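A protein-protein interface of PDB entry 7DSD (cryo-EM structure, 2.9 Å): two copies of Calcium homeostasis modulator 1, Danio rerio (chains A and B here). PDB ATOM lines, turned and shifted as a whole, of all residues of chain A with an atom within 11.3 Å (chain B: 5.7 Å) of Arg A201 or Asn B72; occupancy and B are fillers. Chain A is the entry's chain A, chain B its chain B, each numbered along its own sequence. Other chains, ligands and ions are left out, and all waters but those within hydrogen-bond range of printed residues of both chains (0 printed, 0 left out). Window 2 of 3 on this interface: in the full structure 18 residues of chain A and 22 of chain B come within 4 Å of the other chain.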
ATOM      1  N   TYR A  97     -36.882  -8.606 -14.384  1.00  0.00           N
ATOM      2  CA  TYR A  97     -35.637  -7.949 -14.003  1.00  0.00           C
ATOM      3  C   TYR A  97     -35.161  -8.413 -12.632  1.00  0.00           C
ATOM      4  O   TYR A  97     -34.015  -8.853 -12.480  1.00  0.00           O
ATOM      5  CB  TYR A  97     -35.809  -6.433 -14.016  1.00  0.00           C
ATOM      6  CG  TYR A  97     -34.685  -5.716 -13.311  1.00  0.00           C
ATOM      7  CD1 TYR A  97     -33.432  -5.608 -13.896  1.00  0.00           C
ATOM      8  CD2 TYR A  97     -34.871  -5.156 -12.055  1.00  0.00           C
ATOM      9  CE1 TYR A  97     -32.397  -4.959 -13.255  1.00  0.00           C
ATOM     10  CE2 TYR A  97     -33.842  -4.505 -11.405  1.00  0.00           C
ATOM     11  CZ  TYR A  97     -32.608  -4.409 -12.010  1.00  0.00           C
ATOM     12  OH  TYR A  97     -31.580  -3.760 -11.367  1.00  0.00           O
ATOM     13  N   GLN A 104     -28.794 -14.238 -10.834  1.00  0.00           N
ATOM     14  CA  GLN A 104     -27.381 -13.922 -10.993  1.00  0.00           C
ATOM     15  C   GLN A 104     -26.681 -13.830  -9.645  1.00  0.00           C
ATOM     16  O   GLN A 104     -25.585 -14.375  -9.472  1.00  0.00           O
ATOM     17  CB  GLN A 104     -27.226 -12.622 -11.776  1.00  0.00           C
ATOM     18  CG  GLN A 104     -27.683 -12.731 -13.217  1.00  0.00           C
ATOM     19  CD  GLN A 104     -27.886 -11.380 -13.859  1.00  0.00           C
ATOM     20  OE1 GLN A 104     -27.716 -10.344 -13.216  1.00  0.00           O
ATOM     21  NE2 GLN A 104     -28.253 -11.379 -15.135  1.00  0.00           N
ATOM     22  N   ARG A 105     -27.293 -13.142  -8.677  1.00  0.00           N
ATOM     23  CA  ARG A 105     -26.710 -13.088  -7.342  1.00  0.00           C
ATOM     24  C   ARG A 105     -26.559 -14.477  -6.737  1.00  0.00           C
ATOM     25  O   ARG A 105     -25.586 -14.740  -6.024  1.00  0.00           O
ATOM     26  CB  ARG A 105     -27.566 -12.212  -6.428  1.00  0.00           C
ATOM     27  CG  ARG A 105     -26.954 -10.866  -6.104  1.00  0.00           C
ATOM     28  CD  ARG A 105     -26.653 -10.083  -7.366  1.00  0.00           C
ATOM     29  NE  ARG A 105     -26.007  -8.808  -7.072  1.00  0.00           N
ATOM     30  CZ  ARG A 105     -25.648  -7.926  -7.997  1.00  0.00           C
ATOM     31  NH1 ARG A 105     -25.873  -8.182  -9.279  1.00  0.00           N
ATOM     32  NH2 ARG A 105     -25.065  -6.790  -7.643  1.00  0.00           N
ATOM     33  N   ILE A 108     -23.405 -17.114  -7.782  1.00  0.00           N
ATOM     34  CA  ILE A 108     -22.012 -16.818  -7.456  1.00  0.00           C
ATOM     35  C   ILE A 108     -21.397 -17.948  -6.641  1.00  0.00           C
ATOM     36  O   ILE A 108     -20.369 -18.519  -7.020  1.00  0.00           O
ATOM     37  CB  ILE A 108     -21.902 -15.476  -6.717  1.00  0.00           C
ATOM     38  CG1 ILE A 108     -22.301 -14.328  -7.642  1.00  0.00           C
ATOM     39  CG2 ILE A 108     -20.494 -15.277  -6.201  1.00  0.00           C
ATOM     40  CD1 ILE A 108     -22.196 -12.970  -7.001  1.00  0.00           C
ATOM     41  N   VAL A 192     -13.496 -19.901 -18.762  1.00  0.00           N
ATOM     42  CA  VAL A 192     -14.774 -19.885 -19.471  1.00  0.00           C
ATOM     43  C   VAL A 192     -15.794 -19.043 -18.713  1.00  0.00           C
ATOM     44  O   VAL A 192     -16.541 -18.253 -19.305  1.00  0.00           O
ATOM     45  CB  VAL A 192     -15.279 -21.318 -19.698  1.00  0.00           C
ATOM     46  CG1 VAL A 192     -16.657 -21.295 -20.311  1.00  0.00           C
ATOM     47  CG2 VAL A 192     -14.319 -22.074 -20.589  1.00  0.00           C
ATOM     48  N   ILE A 193     -15.840 -19.201 -17.388  1.00  0.00           N
ATOM     49  CA  ILE A 193     -16.773 -18.421 -16.579  1.00  0.00           C
ATOM     50  C   ILE A 193     -16.502 -16.931 -16.733  1.00  0.00           C
ATOM     51  O   ILE A 193     -17.433 -16.128 -16.897  1.00  0.00           O
ATOM     52  CB  ILE A 193     -16.697 -18.864 -15.107  1.00  0.00           C
ATOM     53  CG1 ILE A 193     -17.319 -20.245 -14.942  1.00  0.00           C
ATOM     54  CG2 ILE A 193     -17.395 -17.871 -14.209  1.00  0.00           C
ATOM     55  CD1 ILE A 193     -18.724 -20.328 -15.470  1.00  0.00           C
ATOM     56  N   THR A 194     -15.229 -16.534 -16.685  1.00  0.00           N
ATOM     57  CA  THR A 194     -14.912 -15.113 -16.778  1.00  0.00           C
ATOM     58  C   THR A 194     -15.236 -14.561 -18.160  1.00  0.00           C
ATOM     59  O   THR A 194     -15.710 -13.427 -18.285  1.00  0.00           O
ATOM     60  CB  THR A 194     -13.446 -14.875 -16.431  1.00  0.00           C
ATOM     61  OG1 THR A 194     -13.175 -15.411 -15.131  1.00  0.00           O
ATOM     62  CG2 THR A 194     -13.143 -13.393 -16.416  1.00  0.00           C
ATOM     63  N   LEU A 195     -15.003 -15.348 -19.213  1.00  0.00           N
ATOM     64  CA  LEU A 195     -15.376 -14.895 -20.551  1.00  0.00           C
ATOM     65  C   LEU A 195     -16.883 -14.694 -20.667  1.00  0.00           C
ATOM     66  O   LEU A 195     -17.345 -13.710 -21.263  1.00  0.00           O
ATOM     67  CB  LEU A 195     -14.892 -15.890 -21.600  1.00  0.00           C
ATOM     68  CG  LEU A 195     -13.426 -15.785 -22.007  1.00  0.00           C
ATOM     69  CD1 LEU A 195     -13.091 -16.853 -23.024  1.00  0.00           C
ATOM     70  CD2 LEU A 195     -13.144 -14.406 -22.566  1.00  0.00           C
ATOM     71  N   VAL A 196     -17.667 -15.623 -20.114  1.00  0.00           N
ATOM     72  CA  VAL A 196     -19.118 -15.481 -20.165  1.00  0.00           C
ATOM     73  C   VAL A 196     -19.558 -14.229 -19.416  1.00  0.00           C
ATOM     74  O   VAL A 196     -20.416 -13.473 -19.892  1.00  0.00           O
ATOM     75  CB  VAL A 196     -19.800 -16.742 -19.606  1.00  0.00           C
ATOM     76  CG1 VAL A 196     -21.286 -16.511 -19.448  1.00  0.00           C
ATOM     77  CG2 VAL A 196     -19.546 -17.919 -20.521  1.00  0.00           C
ATOM     78  N   ALA A 197     -18.982 -13.992 -18.236  1.00  0.00           N
ATOM     79  CA  ALA A 197     -19.332 -12.790 -17.485  1.00  0.00           C
ATOM     80  C   ALA A 197     -18.963 -11.534 -18.260  1.00  0.00           C
ATOM     81  O   ALA A 197     -19.707 -10.545 -18.250  1.00  0.00           O
ATOM     82  CB  ALA A 197     -18.645 -12.802 -16.121  1.00  0.00           C
ATOM     83  N   PHE A 198     -17.817 -11.558 -18.941  1.00  0.00           N
ATOM     84  CA  PHE A 198     -17.399 -10.421 -19.751  1.00  0.00           C
ATOM     85  C   PHE A 198     -18.415 -10.128 -20.844  1.00  0.00           C
ATOM     86  O   PHE A 198     -18.820  -8.976 -21.039  1.00  0.00           O
ATOM     87  CB  PHE A 198     -16.020 -10.694 -20.350  1.00  0.00           C
ATOM     88  CG  PHE A 198     -15.481  -9.572 -21.182  1.00  0.00           C
ATOM     89  CD1 PHE A 198     -14.758  -8.548 -20.601  1.00  0.00           C
ATOM     90  CD2 PHE A 198     -15.685  -9.548 -22.550  1.00  0.00           C
ATOM     91  CE1 PHE A 198     -14.256  -7.517 -21.366  1.00  0.00           C
ATOM     92  CE2 PHE A 198     -15.186  -8.518 -23.319  1.00  0.00           C
ATOM     93  CZ  PHE A 198     -14.472  -7.503 -22.728  1.00  0.00           C
ATOM     94  N   LEU A 199     -18.830 -11.162 -21.578  1.00  0.00           N
ATOM     95  CA  LEU A 199     -19.816 -10.957 -22.635  1.00  0.00           C
ATOM     96  C   LEU A 199     -21.127 -10.423 -22.072  1.00  0.00           C
ATOM     97  O   LEU A 199     -21.732  -9.508 -22.647  1.00  0.00           O
ATOM     98  CB  LEU A 199     -20.058 -12.257 -23.397  1.00  0.00           C
ATOM     99  CG  LEU A 199     -18.889 -12.756 -24.241  1.00  0.00           C
ATOM    100  CD1 LEU A 199     -19.329 -13.908 -25.120  1.00  0.00           C
ATOM    101  CD2 LEU A 199     -18.319 -11.626 -25.076  1.00  0.00           C
ATOM    102  N   VAL A 200     -21.584 -10.983 -20.951  1.00  0.00           N
ATOM    103  CA  VAL A 200     -22.852 -10.549 -20.369  1.00  0.00           C
ATOM    104  C   VAL A 200     -22.785  -9.080 -19.972  1.00  0.00           C
ATOM    105  O   VAL A 200     -23.724  -8.313 -20.210  1.00  0.00           O
ATOM    106  CB  VAL A 200     -23.229 -11.441 -19.174  1.00  0.00           C
ATOM    107  CG1 VAL A 200     -24.365 -10.820 -18.387  1.00  0.00           C
ATOM    108  CG2 VAL A 200     -23.619 -12.821 -19.661  1.00  0.00           C
ATOM    109  N   ARG A 201     -21.672  -8.661 -19.365  1.00  0.00           N
ATOM    110  CA  ARG A 201     -21.572  -7.266 -18.947  1.00  0.00           C
ATOM    111  C   ARG A 201     -21.357  -6.330 -20.129  1.00  0.00           C
ATOM    112  O   ARG A 201     -21.749  -5.161 -20.064  1.00  0.00           O
ATOM    113  CB  ARG A 201     -20.449  -7.087 -17.930  1.00  0.00           C
ATOM    114  CG  ARG A 201     -20.875  -7.313 -16.496  1.00  0.00           C
ATOM    115  CD  ARG A 201     -19.816  -6.818 -15.537  1.00  0.00           C
ATOM    116  NE  ARG A 201     -19.757  -5.362 -15.496  1.00  0.00           N
ATOM    117  CZ  ARG A 201     -20.198  -4.630 -14.481  1.00  0.00           C
ATOM    118  NH1 ARG A 201     -20.109  -3.310 -14.525  1.00  0.00           N
ATOM    119  NH2 ARG A 201     -20.718  -5.219 -13.416  1.00  0.00           N
ATOM    120  N   ALA A 202     -20.747  -6.811 -21.212  1.00  0.00           N
ATOM    121  CA  ALA A 202     -20.457  -5.936 -22.338  1.00  0.00           C
ATOM    122  C   ALA A 202     -21.596  -5.844 -23.343  1.00  0.00           C
ATOM    123  O   ALA A 202     -21.603  -4.914 -24.156  1.00  0.00           O
ATOM    124  CB  ALA A 202     -19.185  -6.399 -23.052  1.00  0.00           C
ATOM    125  N   ILE A 203     -22.555  -6.766 -23.317  1.00  0.00           N
ATOM    126  CA  ILE A 203     -23.681  -6.756 -24.252  1.00  0.00           C
ATOM    127  C   ILE A 203     -24.932  -6.170 -23.606  1.00  0.00           C
ATOM    128  O   ILE A 203     -25.478  -5.173 -24.083  1.00  0.00           O
ATOM    129  CB  ILE A 203     -23.951  -8.168 -24.815  1.00  0.00           C
ATOM    130  CG1 ILE A 203     -22.759  -8.644 -25.646  1.00  0.00           C
ATOM    131  CG2 ILE A 203     -25.223  -8.174 -25.643  1.00  0.00           C
ATOM    132  CD1 ILE A 203     -22.386  -7.709 -26.768  1.00  0.00           C
ATOM    133  N   ARG A 204     -25.401  -6.776 -22.521  1.00  0.00           N
ATOM    134  CA  ARG A 204     -26.624  -6.329 -21.861  1.00  0.00           C
ATOM    135  C   ARG A 204     -26.320  -5.378 -20.709  1.00  0.00           C
ATOM    136  O   ARG A 204     -25.742  -4.308 -20.911  1.00  0.00           O
ATOM    137  CB  ARG A 204     -27.424  -7.531 -21.357  1.00  0.00           C
ATOM    138  CG  ARG A 204     -27.887  -8.471 -22.456  1.00  0.00           C
ATOM    139  CD  ARG A 204     -28.122  -9.878 -21.928  1.00  0.00           C
ATOM    140  NE  ARG A 204     -29.089  -9.911 -20.833  1.00  0.00           N
ATOM    141  CZ  ARG A 204     -30.389 -10.137 -20.989  1.00  0.00           C
ATOM    142  NH1 ARG A 204     -30.888 -10.350 -22.200  1.00  0.00           N
ATOM    143  NH2 ARG A 204     -31.193 -10.148 -19.933  1.00  0.00           N
ATOM    144  N   VAL B  69     -13.475  -6.884 -16.216  1.00  0.00           N
ATOM    145  CA  VAL B  69     -14.897  -7.112 -15.977  1.00  0.00           C
ATOM    146  C   VAL B  69     -15.389  -6.304 -14.784  1.00  0.00           C
ATOM    147  O   VAL B  69     -16.463  -5.696 -14.833  1.00  0.00           O
ATOM    148  CB  VAL B  69     -15.166  -8.615 -15.785  1.00  0.00           C
ATOM    149  CG1 VAL B  69     -16.529  -8.833 -15.174  1.00  0.00           C
ATOM    150  CG2 VAL B  69     -15.063  -9.336 -17.108  1.00  0.00           C
ATOM    151  N   MET B  70     -14.614  -6.268 -13.700  1.00  0.00           N
ATOM    152  CA  MET B  70     -15.102  -5.651 -12.470  1.00  0.00           C
ATOM    153  C   MET B  70     -15.158  -4.132 -12.539  1.00  0.00           C
ATOM    154  O   MET B  70     -15.510  -3.502 -11.537  1.00  0.00           O
ATOM    155  CB  MET B  70     -14.230  -6.070 -11.286  1.00  0.00           C
ATOM    156  CG  MET B  70     -14.291  -7.548 -10.966  1.00  0.00           C
ATOM    157  SD  MET B  70     -13.308  -7.980  -9.521  1.00  0.00           S
ATOM    158  CE  MET B  70     -14.135  -7.025  -8.253  1.00  0.00           C
ATOM    159  N   ASN B  71     -14.823  -3.529 -13.675  1.00  0.00           N
ATOM    160  CA  ASN B  71     -14.859  -2.077 -13.801  1.00  0.00           C
ATOM    161  C   ASN B  71     -16.209  -1.647 -14.359  1.00  0.00           C
ATOM    162  O   ASN B  71     -16.631  -2.128 -15.416  1.00  0.00           O
ATOM    163  CB  ASN B  71     -13.725  -1.587 -14.695  1.00  0.00           C
ATOM    164  CG  ASN B  71     -13.151  -0.270 -14.226  1.00  0.00           C
ATOM    165  OD1 ASN B  71     -13.807   0.481 -13.507  1.00  0.00           O
ATOM    166  ND2 ASN B  71     -11.919   0.013 -14.622  1.00  0.00           N
ATOM    167  N   ASN B  72     -16.874  -0.734 -13.664  1.00  0.00           N
ATOM    168  CA  ASN B  72     -18.248  -0.351 -13.982  1.00  0.00           C
ATOM    169  C   ASN B  72     -18.375   0.488 -15.231  1.00  0.00           C
ATOM    170  O   ASN B  72     -19.484   0.976 -15.468  1.00  0.00           O
ATOM    171  CB  ASN B  72     -18.861   0.399 -12.804  1.00  0.00           C
ATOM    172  CG  ASN B  72     -18.816  -0.401 -11.524  1.00  0.00           C
ATOM    173  OD1 ASN B  72     -19.724  -1.176 -11.231  1.00  0.00           O
ATOM    174  ND2 ASN B  72     -17.753  -0.217 -10.751  1.00  0.00           N
ATOM    175  N   ASN B  73     -17.348   0.702 -16.050  1.00  0.00           N
ATOM    176  CA  ASN B  73     -17.483   1.531 -17.242  1.00  0.00           C
ATOM    177  C   ASN B  73     -17.172   0.763 -18.520  1.00  0.00           C
ATOM    178  O   ASN B  73     -16.690   1.353 -19.491  1.00  0.00           O
ATOM    179  CB  ASN B  73     -16.591   2.768 -17.139  1.00  0.00           C
ATOM    180  CG  ASN B  73     -17.093   3.761 -16.121  1.00  0.00           C
ATOM    181  OD1 ASN B  73     -18.275   3.776 -15.786  1.00  0.00           O
ATOM    182  ND2 ASN B  73     -16.198   4.603 -15.622  1.00  0.00           N
ATOM    183  N   ILE B  74     -17.433  -0.545 -18.545  1.00  0.00           N
ATOM    184  CA  ILE B  74     -17.348  -1.269 -19.808  1.00  0.00           C
ATOM    185  C   ILE B  74     -18.639  -1.112 -20.590  1.00  0.00           C
ATOM    186  O   ILE B  74     -18.633  -1.119 -21.828  1.00  0.00           O
ATOM    187  CB  ILE B  74     -17.020  -2.752 -19.565  1.00  0.00           C
ATOM    188  CG1 ILE B  74     -18.115  -3.409 -18.731  1.00  0.00           C
ATOM    189  CG2 ILE B  74     -15.664  -2.900 -18.907  1.00  0.00           C
ATOM    190  CD1 ILE B  74     -17.974  -4.903 -18.635  1.00  0.00           C
ATOM    191  N   SER B  75     -19.764  -0.968 -19.887  1.00  0.00           N
ATOM    192  CA  SER B  75     -21.045  -0.789 -20.558  1.00  0.00           C
ATOM    193  C   SER B  75     -21.051   0.483 -21.394  1.00  0.00           C
ATOM    194  O   SER B  75     -21.468   0.474 -22.556  1.00  0.00           O
ATOM    195  CB  SER B  75     -22.171  -0.764 -19.525  1.00  0.00           C
ATOM    196  OG  SER B  75     -21.971   0.277 -18.585  1.00  0.00           O
ATOM    197  N   VAL B  76     -20.590   1.594 -20.812  1.00  0.00           N
ATOM    198  CA  VAL B  76     -20.565   2.852 -21.546  1.00  0.00           C
ATOM    199  C   VAL B  76     -19.614   2.770 -22.733  1.00  0.00           C
ATOM    200  O   VAL B  76     -19.923   3.278 -23.818  1.00  0.00           O
ATOM    201  CB  VAL B  76     -20.201   4.015 -20.602  1.00  0.00           C
ATOM    202  CG1 VAL B  76     -21.331   4.261 -19.618  1.00  0.00           C
ATOM    203  CG2 VAL B  76     -18.916   3.719 -19.856  1.00  0.00           C
ATOM    204  N   THR B  78     -18.817   0.097 -24.483  1.00  0.00           N
ATOM    205  CA  THR B  78     -19.467  -0.694 -25.521  1.00  0.00           C
ATOM    206  C   THR B  78     -20.564   0.103 -26.214  1.00  0.00           C
ATOM    207  O   THR B  78     -20.687   0.066 -27.445  1.00  0.00           O
ATOM    208  CB  THR B  78     -20.038  -1.978 -24.926  1.00  0.00           C
ATOM    209  OG1 THR B  78     -20.827  -1.657 -23.774  1.00  0.00           O
ATOM    210  CG2 THR B  78     -18.918  -2.921 -24.529  1.00  0.00           C
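The side-chain hydroxyl (OG1) of Thr B78 sits at hydrogen-bond distance from the backbone carbonyl oxygen (O) of Ile B74, at 3.0 Å.
The backbone carbonyl oxygen (O) of Ser B75 sits at hydrogen-bond distance from the side-chain hydroxyl (OG1) of Thr B78 (2.5 Å).
Of the 17 printed residues of chain A, 3 touch a printed residue of chain B.
Hydrophobic or aromatic side chains of chain A that line the printed part of chain B: Phe A198 and Ala A202.
Printed residues of chain B that touch a printed residue of chain A: Val B69, Asn B71, Asn B72, Ile B74 and Thr B78.
Among the printed residues, 6 pairs touch across the chains.
Among the printed residues, no Asp or Glu carboxylate lies within 4 Å of a Lys or Arg side-chain nitrogen of the other chain.
CD1 of Phe A198 touches CG2 of Val B69 (3.6 Å).
Asn B71 touches Arg A201 (O to NH1, 3.8 Å).
CA of Asn B72 touches NH1 of Arg A201, at 3.5 Å.
CB of Arg A201 touches CD1 of Ile B74 (3.4 Å).
The backbone carbonyl oxygen of Ala A202 lies close to the side-chain hydroxyl of Thr B78, at 3.4 Å.
The backbone carbonyl oxygen (O) of Val B69 sits at hydrogen-bond distance from the guanidinium group (NE) of Arg A201 (3.4 Å).
Printed residues of chain B within 4 Å of Phe A198: Val B69.
Of chain B, only Val B69, Asn B71, Asn B72 and Ile B74 come within 4 Å of Arg A201.
Of the printed residues of chain B, Ala A202 touches Thr B78.
Val B69 touches just these residues of chain A: Phe A198 (3.6 Å) and Arg A201 (3.4 Å).
Asn B71 touches just one residue of chain A: Arg A201 (3.8 Å).
Asn B72 touches just one residue of chain A: Arg A201 (3.5 Å).
Asn B73 touches none of the printed residues of chain A.
Of the printed residues of chain A, Thr B78 touches Ala A202 (3.4 Å).
The nearest residue of chain A that does not touch Asn B72 is Arg A105 (8.5 Å).
No position is printed for both chains.
Of the 6 pairs that touch across the chains among the printed residues, none has its exchanged pair printed and touching as well.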
